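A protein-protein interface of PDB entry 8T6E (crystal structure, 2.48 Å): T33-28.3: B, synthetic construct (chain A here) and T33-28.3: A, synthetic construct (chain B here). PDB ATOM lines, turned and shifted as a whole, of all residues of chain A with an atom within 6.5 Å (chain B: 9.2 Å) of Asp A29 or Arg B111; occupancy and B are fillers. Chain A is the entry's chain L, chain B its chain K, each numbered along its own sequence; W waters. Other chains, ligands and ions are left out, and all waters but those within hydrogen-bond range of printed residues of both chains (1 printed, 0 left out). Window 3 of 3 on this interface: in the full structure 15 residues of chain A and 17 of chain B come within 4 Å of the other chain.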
ATOM      1  N   TYR A  24     -12.576 -16.609   6.639  1.00  0.00           N
ATOM      2  CA  TYR A  24     -13.010 -17.398   7.787  1.00  0.00           C
ATOM      3  C   TYR A  24     -12.712 -18.879   7.586  1.00  0.00           C
ATOM      4  O   TYR A  24     -12.382 -19.588   8.544  1.00  0.00           O
ATOM      5  CB  TYR A  24     -14.500 -17.181   8.048  1.00  0.00           C
ATOM      6  CG  TYR A  24     -14.852 -15.805   8.574  1.00  0.00           C
ATOM      7  CD1 TYR A  24     -13.880 -14.979   9.123  1.00  0.00           C
ATOM      8  CD2 TYR A  24     -16.158 -15.336   8.526  1.00  0.00           C
ATOM      9  CE1 TYR A  24     -14.198 -13.723   9.605  1.00  0.00           C
ATOM     10  CE2 TYR A  24     -16.487 -14.081   9.006  1.00  0.00           C
ATOM     11  CZ  TYR A  24     -15.503 -13.278   9.544  1.00  0.00           C
ATOM     12  OH  TYR A  24     -15.822 -12.028  10.023  1.00  0.00           O
ATOM     13  N   ARG A  25     -12.827 -19.369   6.347  1.00  0.00           N
ATOM     14  CA  ARG A  25     -12.456 -20.753   6.068  1.00  0.00           C
ATOM     15  C   ARG A  25     -10.966 -20.978   6.296  1.00  0.00           C
ATOM     16  O   ARG A  25     -10.554 -22.051   6.750  1.00  0.00           O
ATOM     17  CB  ARG A  25     -12.844 -21.132   4.636  1.00  0.00           C
ATOM     18  CG  ARG A  25     -14.331 -21.398   4.444  1.00  0.00           C
ATOM     19  CD  ARG A  25     -14.679 -21.779   3.007  1.00  0.00           C
ATOM     20  NE  ARG A  25     -14.069 -23.035   2.584  1.00  0.00           N
ATOM     21  CZ  ARG A  25     -13.155 -23.141   1.629  1.00  0.00           C
ATOM     22  NH1 ARG A  25     -12.725 -22.081   0.963  1.00  0.00           N
ATOM     23  NH2 ARG A  25     -12.666 -24.341   1.329  1.00  0.00           N
ATOM     24  N   ILE A  26     -10.143 -19.974   5.988  1.00  0.00           N
ATOM     25  CA  ILE A  26      -8.710 -20.085   6.241  1.00  0.00           C
ATOM     26  C   ILE A  26      -8.434 -20.080   7.739  1.00  0.00           C
ATOM     27  O   ILE A  26      -7.649 -20.890   8.246  1.00  0.00           O
ATOM     28  CB  ILE A  26      -7.952 -18.951   5.528  1.00  0.00           C
ATOM     29  CG1 ILE A  26      -8.197 -19.009   4.018  1.00  0.00           C
ATOM     30  CG2 ILE A  26      -6.466 -19.031   5.834  1.00  0.00           C
ATOM     31  CD1 ILE A  26      -7.766 -17.759   3.279  1.00  0.00           C
ATOM     32  N   VAL A  27      -9.078 -19.165   8.470  1.00  0.00           N
ATOM     33  CA  VAL A  27      -8.869 -19.067   9.913  1.00  0.00           C
ATOM     34  C   VAL A  27      -9.274 -20.364  10.601  1.00  0.00           C
ATOM     35  O   VAL A  27      -8.612 -20.819  11.543  1.00  0.00           O
ATOM     36  CB  VAL A  27      -9.641 -17.862  10.482  1.00  0.00           C
ATOM     37  CG1 VAL A  27      -9.526 -17.820  11.999  1.00  0.00           C
ATOM     38  CG2 VAL A  27      -9.130 -16.570   9.872  1.00  0.00           C
ATOM     39  N   THR A  28     -10.362 -20.982  10.139  1.00  0.00           N
ATOM     40  CA  THR A  28     -10.825 -22.223  10.749  1.00  0.00           C
ATOM     41  C   THR A  28      -9.837 -23.360  10.516  1.00  0.00           C
ATOM     42  O   THR A  28      -9.568 -24.152  11.428  1.00  0.00           O
ATOM     43  CB  THR A  28     -12.205 -22.590  10.202  1.00  0.00           C
ATOM     44  OG1 THR A  28     -13.127 -21.527  10.473  1.00  0.00           O
ATOM     45  CG2 THR A  28     -12.715 -23.871  10.847  1.00  0.00           C
ATOM     46  N   ASP A  29      -9.277 -23.453   9.309  1.00  0.00           N
ATOM     47  CA  ASP A  29      -8.420 -24.585   8.971  1.00  0.00           C
ATOM     48  C   ASP A  29      -7.024 -24.447   9.570  1.00  0.00           C
ATOM     49  O   ASP A  29      -6.492 -25.410  10.132  1.00  0.00           O
ATOM     50  CB  ASP A  29      -8.342 -24.745   7.451  1.00  0.00           C
ATOM     51  CG  ASP A  29      -7.304 -25.770   7.019  1.00  0.00           C
ATOM     52  OD1 ASP A  29      -6.103 -25.428   6.977  1.00  0.00           O
ATOM     53  OD2 ASP A  29      -7.690 -26.922   6.727  1.00  0.00           O
ATOM     54  N   THR A  30      -6.418 -23.266   9.459  1.00  0.00           N
ATOM     55  CA  THR A  30      -5.032 -23.071   9.879  1.00  0.00           C
ATOM     56  C   THR A  30      -4.914 -22.799  11.378  1.00  0.00           C
ATOM     57  O   THR A  30      -4.205 -23.516  12.092  1.00  0.00           O
ATOM     58  CB  THR A  30      -4.391 -21.928   9.077  1.00  0.00           C
ATOM     59  OG1 THR A  30      -5.034 -20.692   9.404  1.00  0.00           O
ATOM     60  CG2 THR A  30      -4.525 -22.179   7.582  1.00  0.00           C
ATOM     61  N   ILE A  31      -5.603 -21.767  11.867  1.00  0.00           N
ATOM     62  CA  ILE A  31      -5.435 -21.358  13.259  1.00  0.00           C
ATOM     63  C   ILE A  31      -6.217 -22.270  14.196  1.00  0.00           C
ATOM     64  O   ILE A  31      -5.671 -22.794  15.174  1.00  0.00           O
ATOM     65  CB  ILE A  31      -5.845 -19.884  13.436  1.00  0.00           C
ATOM     66  CG1 ILE A  31      -5.088 -19.000  12.444  1.00  0.00           C
ATOM     67  CG2 ILE A  31      -5.581 -19.430  14.862  1.00  0.00           C
ATOM     68  CD1 ILE A  31      -5.491 -17.541  12.489  1.00  0.00           C
ATOM     69  N   LEU A  32      -7.508 -22.472  13.921  1.00  0.00           N
ATOM     70  CA  LEU A  32      -8.340 -23.279  14.806  1.00  0.00           C
ATOM     71  C   LEU A  32      -8.083 -24.774  14.668  1.00  0.00           C
ATOM     72  O   LEU A  32      -8.479 -25.538  15.554  1.00  0.00           O
ATOM     73  CB  LEU A  32      -9.821 -22.992  14.555  1.00  0.00           C
ATOM     74  CG  LEU A  32     -10.313 -21.592  14.930  1.00  0.00           C
ATOM     75  CD1 LEU A  32     -11.832 -21.538  14.901  1.00  0.00           C
ATOM     76  CD2 LEU A  32      -9.780 -21.178  16.295  1.00  0.00           C
ATOM     77  N   GLY A  33      -7.435 -25.206  13.589  1.00  0.00           N
ATOM     78  CA  GLY A  33      -7.155 -26.619  13.406  1.00  0.00           C
ATOM     79  C   GLY A  33      -8.383 -27.480  13.215  1.00  0.00           C
ATOM     80  O   GLY A  33      -8.361 -28.665  13.562  1.00  0.00           O
ATOM     81  N   LYS A  34      -9.457 -26.916  12.679  1.00  0.00           N
ATOM     82  CA  LYS A  34     -10.706 -27.614  12.435  1.00  0.00           C
ATOM     83  C   LYS A  34     -11.055 -27.546  10.953  1.00  0.00           C
ATOM     84  O   LYS A  34     -10.598 -26.646  10.240  1.00  0.00           O
ATOM     85  CB  LYS A  34     -11.842 -27.006  13.272  1.00  0.00           C
ATOM     86  CG  LYS A  34     -11.628 -27.113  14.774  1.00  0.00           C
ATOM     87  CD  LYS A  34     -11.481 -28.563  15.209  1.00  0.00           C
ATOM     88  CE  LYS A  34     -11.264 -28.673  16.710  1.00  0.00           C
ATOM     89  NZ  LYS A  34     -11.126 -30.089  17.152  1.00  0.00           N
ATOM     90  N   PRO A  35     -11.850 -28.494  10.450  1.00  0.00           N
ATOM     91  CA  PRO A  35     -12.182 -28.493   9.019  1.00  0.00           C
ATOM     92  C   PRO A  35     -12.920 -27.226   8.613  1.00  0.00           C
ATOM     93  O   PRO A  35     -13.807 -26.744   9.321  1.00  0.00           O
ATOM     94  CB  PRO A  35     -13.067 -29.734   8.860  1.00  0.00           C
ATOM     95  CG  PRO A  35     -12.687 -30.618   9.998  1.00  0.00           C
ATOM     96  CD  PRO A  35     -12.372 -29.690  11.134  1.00  0.00           C
ATOM     97  N   ALA A  36     -12.544 -26.690   7.448  1.00  0.00           N
ATOM     98  CA  ALA A  36     -13.129 -25.452   6.946  1.00  0.00           C
ATOM     99  C   ALA A  36     -14.570 -25.615   6.481  1.00  0.00           C
ATOM    100  O   ALA A  36     -15.234 -24.608   6.214  1.00  0.00           O
ATOM    101  CB  ALA A  36     -12.276 -24.898   5.802  1.00  0.00           C
ATOM    102  N   ALA B  53      -6.402 -15.135   0.636  1.00  0.00           N
ATOM    103  CA  ALA B  53      -5.169 -15.607   1.258  1.00  0.00           C
ATOM    104  C   ALA B  53      -4.279 -14.448   1.684  1.00  0.00           C
ATOM    105  O   ALA B  53      -3.530 -14.564   2.661  1.00  0.00           O
ATOM    106  CB  ALA B  53      -4.416 -16.532   0.301  1.00  0.00           C
ATOM    107  N   TYR B  56      -4.901 -13.302   5.186  1.00  0.00           N
ATOM    108  CA  TYR B  56      -4.302 -14.139   6.220  1.00  0.00           C
ATOM    109  C   TYR B  56      -2.894 -13.667   6.551  1.00  0.00           C
ATOM    110  O   TYR B  56      -2.474 -13.710   7.713  1.00  0.00           O
ATOM    111  CB  TYR B  56      -4.289 -15.600   5.772  1.00  0.00           C
ATOM    112  CG  TYR B  56      -3.702 -16.550   6.794  1.00  0.00           C
ATOM    113  CD1 TYR B  56      -4.375 -16.826   7.976  1.00  0.00           C
ATOM    114  CD2 TYR B  56      -2.483 -17.181   6.571  1.00  0.00           C
ATOM    115  CE1 TYR B  56      -3.848 -17.695   8.912  1.00  0.00           C
ATOM    116  CE2 TYR B  56      -1.948 -18.053   7.503  1.00  0.00           C
ATOM    117  CZ  TYR B  56      -2.636 -18.306   8.671  1.00  0.00           C
ATOM    118  OH  TYR B  56      -2.109 -19.173   9.600  1.00  0.00           O
ATOM    119  N   LEU B  57      -2.152 -13.207   5.542  1.00  0.00           N
ATOM    120  CA  LEU B  57      -0.793 -12.731   5.755  1.00  0.00           C
ATOM    121  C   LEU B  57      -0.748 -11.313   6.310  1.00  0.00           C
ATOM    122  O   LEU B  57       0.247 -10.940   6.941  1.00  0.00           O
ATOM    123  CB  LEU B  57      -0.004 -12.800   4.445  1.00  0.00           C
ATOM    124  CG  LEU B  57      -0.018 -14.155   3.733  1.00  0.00           C
ATOM    125  CD1 LEU B  57       0.836 -14.113   2.473  1.00  0.00           C
ATOM    126  CD2 LEU B  57       0.449 -15.260   4.665  1.00  0.00           C
ATOM    127  N   LEU B  91       4.900 -14.717  -4.077  1.00  0.00           N
ATOM    128  CA  LEU B  91       5.035 -14.326  -2.678  1.00  0.00           C
ATOM    129  C   LEU B  91       6.158 -13.300  -2.590  1.00  0.00           C
ATOM    130  O   LEU B  91       7.322 -13.619  -2.853  1.00  0.00           O
ATOM    131  CB  LEU B  91       5.323 -15.532  -1.789  1.00  0.00           C
ATOM    132  CG  LEU B  91       5.480 -15.217  -0.300  1.00  0.00           C
ATOM    133  CD1 LEU B  91       4.206 -14.596   0.261  1.00  0.00           C
ATOM    134  CD2 LEU B  91       5.860 -16.463   0.481  1.00  0.00           C
ATOM    135  N   GLU B 103      10.847 -18.473   5.343  1.00  0.00           N
ATOM    136  CA  GLU B 103      10.207 -19.784   5.395  1.00  0.00           C
ATOM    137  C   GLU B 103       8.875 -19.726   6.133  1.00  0.00           C
ATOM    138  O   GLU B 103       7.925 -20.426   5.763  1.00  0.00           O
ATOM    139  CB  GLU B 103      11.148 -20.800   6.044  1.00  0.00           C
ATOM    140  CG  GLU B 103      12.199 -21.349   5.093  1.00  0.00           C
ATOM    141  CD  GLU B 103      13.313 -22.095   5.806  1.00  0.00           C
ATOM    142  OE1 GLU B 103      13.333 -22.091   7.056  1.00  0.00           O
ATOM    143  OE2 GLU B 103      14.172 -22.683   5.115  1.00  0.00           O
ATOM    144  N   THR B 104       8.783 -18.903   7.182  1.00  0.00           N
ATOM    145  CA  THR B 104       7.508 -18.733   7.870  1.00  0.00           C
ATOM    146  C   THR B 104       6.466 -18.120   6.944  1.00  0.00           C
ATOM    147  O   THR B 104       5.312 -18.568   6.911  1.00  0.00           O
ATOM    148  CB  THR B 104       7.690 -17.869   9.119  1.00  0.00           C
ATOM    149  OG1 THR B 104       8.451 -18.593  10.093  1.00  0.00           O
ATOM    150  CG2 THR B 104       6.343 -17.490   9.716  1.00  0.00           C
ATOM    151  N   ALA B 105       6.857 -17.102   6.174  1.00  0.00           N
ATOM    152  CA  ALA B 105       5.938 -16.509   5.209  1.00  0.00           C
ATOM    153  C   ALA B 105       5.586 -17.485   4.096  1.00  0.00           C
ATOM    154  O   ALA B 105       4.466 -17.453   3.575  1.00  0.00           O
ATOM    155  CB  ALA B 105       6.541 -15.230   4.625  1.00  0.00           C
ATOM    156  N   GLU B 106       6.522 -18.362   3.724  1.00  0.00           N
ATOM    157  CA  GLU B 106       6.247 -19.339   2.676  1.00  0.00           C
ATOM    158  C   GLU B 106       5.207 -20.361   3.124  1.00  0.00           C
ATOM    159  O   GLU B 106       4.323 -20.733   2.345  1.00  0.00           O
ATOM    160  CB  GLU B 106       7.543 -20.032   2.259  1.00  0.00           C
ATOM    161  CG  GLU B 106       8.305 -19.294   1.170  1.00  0.00           C
ATOM    162  CD  GLU B 106       9.768 -19.687   1.103  1.00  0.00           C
ATOM    163  OE1 GLU B 106      10.300 -20.177   2.121  1.00  0.00           O
ATOM    164  OE2 GLU B 106      10.386 -19.505   0.034  1.00  0.00           O
ATOM    165  N   GLU B 107       5.289 -20.822   4.373  1.00  0.00           N
ATOM    166  CA  GLU B 107       4.342 -21.824   4.850  1.00  0.00           C
ATOM    167  C   GLU B 107       2.970 -21.221   5.129  1.00  0.00           C
ATOM    168  O   GLU B 107       1.946 -21.846   4.833  1.00  0.00           O
ATOM    169  CB  GLU B 107       4.890 -22.514   6.102  1.00  0.00           C
ATOM    170  CG  GLU B 107       3.968 -23.580   6.696  1.00  0.00           C
ATOM    171  CD  GLU B 107       3.764 -24.784   5.781  1.00  0.00           C
ATOM    172  OE1 GLU B 107       4.499 -24.916   4.780  1.00  0.00           O
ATOM    173  OE2 GLU B 107       2.864 -25.604   6.064  1.00  0.00           O
ATOM    174  N   ARG B 108       2.929 -20.014   5.701  1.00  0.00           N
ATOM    175  CA  ARG B 108       1.649 -19.355   5.941  1.00  0.00           C
ATOM    176  C   ARG B 108       0.909 -19.101   4.635  1.00  0.00           C
ATOM    177  O   ARG B 108      -0.315 -19.263   4.562  1.00  0.00           O
ATOM    178  CB  ARG B 108       1.865 -18.045   6.698  1.00  0.00           C
ATOM    179  CG  ARG B 108       2.155 -18.224   8.177  1.00  0.00           C
ATOM    180  CD  ARG B 108       2.551 -16.911   8.824  1.00  0.00           C
ATOM    181  NE  ARG B 108       2.760 -17.055  10.260  1.00  0.00           N
ATOM    182  CZ  ARG B 108       3.360 -16.151  11.023  1.00  0.00           C
ATOM    183  NH1 ARG B 108       3.850 -15.034  10.513  1.00  0.00           N
ATOM    184  NH2 ARG B 108       3.475 -16.379  12.328  1.00  0.00           N
ATOM    185  N   ALA B 109       1.638 -18.708   3.589  1.00  0.00           N
ATOM    186  CA  ALA B 109       1.014 -18.503   2.288  1.00  0.00           C
ATOM    187  C   ALA B 109       0.558 -19.824   1.680  1.00  0.00           C
ATOM    188  O   ALA B 109      -0.520 -19.897   1.080  1.00  0.00           O
ATOM    189  CB  ALA B 109       1.982 -17.783   1.350  1.00  0.00           C
ATOM    190  N   ARG B 110       1.361 -20.879   1.831  1.00  0.00           N
ATOM    191  CA  ARG B 110       0.986 -22.176   1.276  1.00  0.00           C
ATOM    192  C   ARG B 110      -0.219 -22.772   1.993  1.00  0.00           C
ATOM    193  O   ARG B 110      -1.033 -23.456   1.364  1.00  0.00           O
ATOM    194  CB  ARG B 110       2.174 -23.135   1.330  1.00  0.00           C
ATOM    195  CG  ARG B 110       3.249 -22.825   0.302  1.00  0.00           C
ATOM    196  CD  ARG B 110       4.429 -23.772   0.411  1.00  0.00           C
ATOM    197  NE  ARG B 110       5.462 -23.433  -0.558  1.00  0.00           N
ATOM    198  CZ  ARG B 110       5.448 -23.811  -1.829  1.00  0.00           C
ATOM    199  NH1 ARG B 110       4.467 -24.553  -2.318  1.00  0.00           N
ATOM    200  NH2 ARG B 110       6.441 -23.435  -2.630  1.00  0.00           N
ATOM    201  N   ARG B 111      -0.353 -22.527   3.298  1.00  0.00           N
ATOM    202  CA  ARG B 111      -1.533 -23.002   4.013  1.00  0.00           C
ATOM    203  C   ARG B 111      -2.778 -22.232   3.587  1.00  0.00           C
ATOM    204  O   ARG B 111      -3.843 -22.825   3.377  1.00  0.00           O
ATOM    205  CB  ARG B 111      -1.323 -22.887   5.523  1.00  0.00           C
ATOM    206  CG  ARG B 111      -0.284 -23.843   6.087  1.00  0.00           C
ATOM    207  CD  ARG B 111      -0.841 -25.249   6.257  1.00  0.00           C
ATOM    208  NE  ARG B 111      -1.361 -25.477   7.601  1.00  0.00           N
ATOM    209  CZ  ARG B 111      -2.649 -25.504   7.917  1.00  0.00           C
ATOM    210  NH1 ARG B 111      -3.588 -25.334   7.001  1.00  0.00           N
ATOM    211  NH2 ARG B 111      -3.002 -25.709   9.182  1.00  0.00           N
ATOM    212  N   ALA B 112      -2.658 -20.911   3.445  1.00  0.00           N
ATOM    213  CA  ALA B 112      -3.807 -20.098   3.056  1.00  0.00           C
ATOM    214  C   ALA B 112      -4.233 -20.385   1.622  1.00  0.00           C
ATOM    215  O   ALA B 112      -5.431 -20.467   1.328  1.00  0.00           O
ATOM    216  CB  ALA B 112      -3.478 -18.617   3.234  1.00  0.00           C
ATOM    217  N   LEU B 113      -3.268 -20.536   0.714  1.00  0.00           N
ATOM    218  CA  LEU B 113      -3.601 -20.802  -0.681  1.00  0.00           C
ATOM    219  C   LEU B 113      -4.219 -22.182  -0.862  1.00  0.00           C
ATOM    220  O   LEU B 113      -5.010 -22.387  -1.788  1.00  0.00           O
ATOM    221  CB  LEU B 113      -2.355 -20.653  -1.551  1.00  0.00           C
ATOM    222  CG  LEU B 113      -1.861 -19.218  -1.758  1.00  0.00           C
ATOM    223  CD1 LEU B 113      -0.464 -19.206  -2.357  1.00  0.00           C
ATOM    224  CD2 LEU B 113      -2.831 -18.446  -2.638  1.00  0.00           C
ATOM    225  N   ALA B 114      -3.873 -23.137   0.005  1.00  0.00           N
ATOM    226  CA  ALA B 114      -4.482 -24.460  -0.083  1.00  0.00           C
ATOM    227  C   ALA B 114      -5.980 -24.392   0.183  1.00  0.00           C
ATOM    228  O   ALA B 114      -6.773 -25.051  -0.502  1.00  0.00           O
ATOM    229  CB  ALA B 114      -3.803 -25.416   0.896  1.00  0.00           C
ATOM    230  N   VAL B 115      -6.389 -23.594   1.169  1.00  0.00           N
ATOM    231  CA  VAL B 115      -7.807 -23.449   1.480  1.00  0.00           C
ATOM    232  C   VAL B 115      -8.494 -22.541   0.468  1.00  0.00           C
ATOM    233  O   VAL B 115      -9.518 -22.908  -0.120  1.00  0.00           O
ATOM    234  CB  VAL B 115      -7.986 -22.923   2.917  1.00  0.00           C
ATOM    235  CG1 VAL B 115      -9.456 -22.655   3.205  1.00  0.00           C
ATOM    236  CG2 VAL B 115      -7.408 -23.903   3.923  1.00  0.00           C
ATOM    237  N   ALA B 116      -7.936 -21.347   0.252  1.00  0.00           N
ATOM    238  CA  ALA B 116      -8.600 -20.341  -0.573  1.00  0.00           C
ATOM    239  C   ALA B 116      -8.759 -20.791  -2.020  1.00  0.00           C
ATOM    240  O   ALA B 116      -9.763 -20.460  -2.661  1.00  0.00           O
ATOM    241  CB  ALA B 116      -7.826 -19.024  -0.514  1.00  0.00           C
ATOM    242  N   LEU B 117      -7.793 -21.531  -2.554  1.00  0.00           N
ATOM    243  CA  LEU B 117      -7.884 -22.034  -3.916  1.00  0.00           C
ATOM    244  C   LEU B 117      -8.489 -23.429  -3.989  1.00  0.00           C
ATOM    245  O   LEU B 117      -8.688 -23.942  -5.096  1.00  0.00           O
ATOM    246  CB  LEU B 117      -6.499 -22.036  -4.572  1.00  0.00           C
ATOM    247  CG  LEU B 117      -5.726 -20.717  -4.493  1.00  0.00           C
ATOM    248  CD1 LEU B 117      -4.385 -20.832  -5.201  1.00  0.00           C
ATOM    249  CD2 LEU B 117      -6.547 -19.571  -5.068  1.00  0.00           C
ATOM    250  N   ARG B 118      -8.783 -24.043  -2.844  1.00  0.00           N
ATOM    251  CA  ARG B 118      -9.386 -25.375  -2.763  1.00  0.00           C
ATOM    252  C   ARG B 118      -8.570 -26.393  -3.559  1.00  0.00           C
ATOM    253  O   ARG B 118      -9.018 -26.951  -4.563  1.00  0.00           O
ATOM    254  CB  ARG B 118     -10.843 -25.346  -3.230  1.00  0.00           C
ATOM    255  CG  ARG B 118     -11.690 -24.270  -2.566  1.00  0.00           C
ATOM    256  CD  ARG B 118     -13.165 -24.447  -2.902  1.00  0.00           C
ATOM    257  NE  ARG B 118     -13.777 -25.526  -2.137  1.00  0.00           N
ATOM    258  CZ  ARG B 118     -14.649 -25.348  -1.153  1.00  0.00           C
ATOM    259  NH1 ARG B 118     -15.066 -24.141  -0.809  1.00  0.00           N
ATOM    260  NH2 ARG B 118     -15.119 -26.409  -0.503  1.00  0.00           N
ATOM    261  N   VAL B 119      -7.355 -26.638  -3.085  1.00  0.00           N
ATOM    262  CA  VAL B 119      -6.422 -27.486  -3.816  1.00  0.00           C
ATOM    263  C   VAL B 119      -6.792 -28.951  -3.634  1.00  0.00           C
ATOM    264  O   VAL B 119      -7.325 -29.361  -2.595  1.00  0.00           O
ATOM    265  CB  VAL B 119      -4.971 -27.212  -3.374  1.00  0.00           C
ATOM    266  CG1 VAL B 119      -4.621 -25.748  -3.588  1.00  0.00           C
ATOM    267  CG2 VAL B 119      -4.771 -27.609  -1.921  1.00  0.00           C
ATOM    268  N   GLU B 121      -9.104 -30.769  -4.832  1.00  0.00           N
ATOM    269  CA  GLU B 121     -10.522 -31.056  -4.679  1.00  0.00           C
ATOM    270  C   GLU B 121     -11.297 -30.223  -5.689  1.00  0.00           C
ATOM    271  O   GLU B 121     -10.826 -29.181  -6.151  1.00  0.00           O
ATOM    272  CB  GLU B 121     -11.014 -30.769  -3.255  1.00  0.00           C
ATOM    273  CG  GLU B 121     -11.093 -29.291  -2.906  1.00  0.00           C
ATOM    274  CD  GLU B 121     -11.609 -29.054  -1.499  1.00  0.00           C
ATOM    275  OE1 GLU B 121     -11.433 -29.946  -0.643  1.00  0.00           O
ATOM    276  OE2 GLU B 121     -12.195 -27.979  -1.251  1.00  0.00           O
ATOM    277  N   PHE B 131      -1.485 -25.054  -7.378  1.00  0.00           N
ATOM    278  CA  PHE B 131      -0.858 -23.745  -7.446  1.00  0.00           C
ATOM    279  C   PHE B 131       0.656 -23.885  -7.385  1.00  0.00           C
ATOM    280  O   PHE B 131       1.197 -24.911  -6.965  1.00  0.00           O
ATOM    281  CB  PHE B 131      -1.364 -22.807  -6.336  1.00  0.00           C
ATOM    282  CG  PHE B 131      -0.800 -23.098  -4.974  1.00  0.00           C
ATOM    283  CD1 PHE B 131      -1.420 -24.006  -4.132  1.00  0.00           C
ATOM    284  CD2 PHE B 131       0.336 -22.444  -4.527  1.00  0.00           C
ATOM    285  CE1 PHE B 131      -0.907 -24.268  -2.873  1.00  0.00           C
ATOM    286  CE2 PHE B 131       0.856 -22.703  -3.273  1.00  0.00           C
ATOM    287  CZ  PHE B 131       0.233 -23.615  -2.445  1.00  0.00           C
ATOM    288  N   MET B 133       4.137 -21.286  -6.433  1.00  0.00           N
ATOM    289  CA  MET B 133       4.457 -20.057  -5.715  1.00  0.00           C
ATOM    290  C   MET B 133       5.914 -19.687  -5.952  1.00  0.00           C
ATOM    291  O   MET B 133       6.819 -20.443  -5.578  1.00  0.00           O
ATOM    292  CB  MET B 133       4.179 -20.218  -4.219  1.00  0.00           C
ATOM    293  CG  MET B 133       4.141 -18.912  -3.441  1.00  0.00           C
ATOM    294  SD  MET B 133       3.797 -19.163  -1.688  1.00  0.00           S
ATOM    295  CE  MET B 133       5.305 -19.970  -1.152  1.00  0.00           C
HETATM  296  O   HOH W   1      -3.843 -26.452  12.054  1.00  0.00           O
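OH of Tyr B56 lies close to OG1 of Thr A30 (3.3 Å). The guanidinium group (NH1) of Arg B111 lies within salt-bridge range of the side-chain carboxylate (OD1) of Asp A29 (2.5 Å). NH1 of Arg A25 sits at hydrogen-bond distance from O of Val B115 (3.5 Å). The guanidinium group (NH1) of Arg B118 sits close to the guanidinium group (NH2) of Arg A25 (3.2 Å).
OE2 of Glu B121 lies within salt-bridge range of NE of Arg B118, at 3.1 Å. The backbone carbonyl oxygen (O) of Ile A26 lies within hydrogen-bond range of the side-chain hydroxyl (OG1) of Thr A30.
Among the printed residues, pairs that only touch across the chains: Ile A26 with Ala B53 (3.9 Å), Ile A26 with Tyr B56 (3.7 Å), Ile A26 with Ala B112 (3.98 Å), Ile A26 with Val B115 (3.9 Å), Ile A26 with Ala B116 (3.999 Å), Asp A29 with Val B115 (3.6 Å), Thr A30 with Arg B111 (3.3 Å) and Ile A31 with Tyr B56 (3.9 Å).
Val A27 touches none of the printed residues of chain B. No residue of chain B comes within 4 Å of Thr A28. Asp A29 touches two residues of chain B. Thr A30 touches two residues of chain B. Printed residues of chain A within 4 Å of Ala B116: Ile A26 (3.999 Å). Of the printed residues of chain A, Arg B118 touches Arg A25 (3.2 Å). The nearest residue of chain B that does not touch Asp A29 is Ala B114 (6.5 Å). The nearest printed residue of chain A that does not touch Ala B53 is Tyr A24 (8.7 Å).
Of the 13 printed residues of chain A, 5 touch a printed residue of chain B. Hydrophobic or aromatic side chains of chain A within 4 Å of the printed part of chain B: Ile A26 and Ile A31. Of the 24 printed residues of chain B, 7 touch a printed residue of chain A. Among the printed residues, 12 pairs touch across the chains. Among the printed residues, Asp or Glu carboxylates within 4 Å of a Lys or Arg side-chain nitrogen of the other chain: Asp A29 with Arg B111 (2.5 Å).
Water W1 lies within hydrogen-bond range of O of Thr A30, NH2 of Arg B111 and O of Asp A29.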
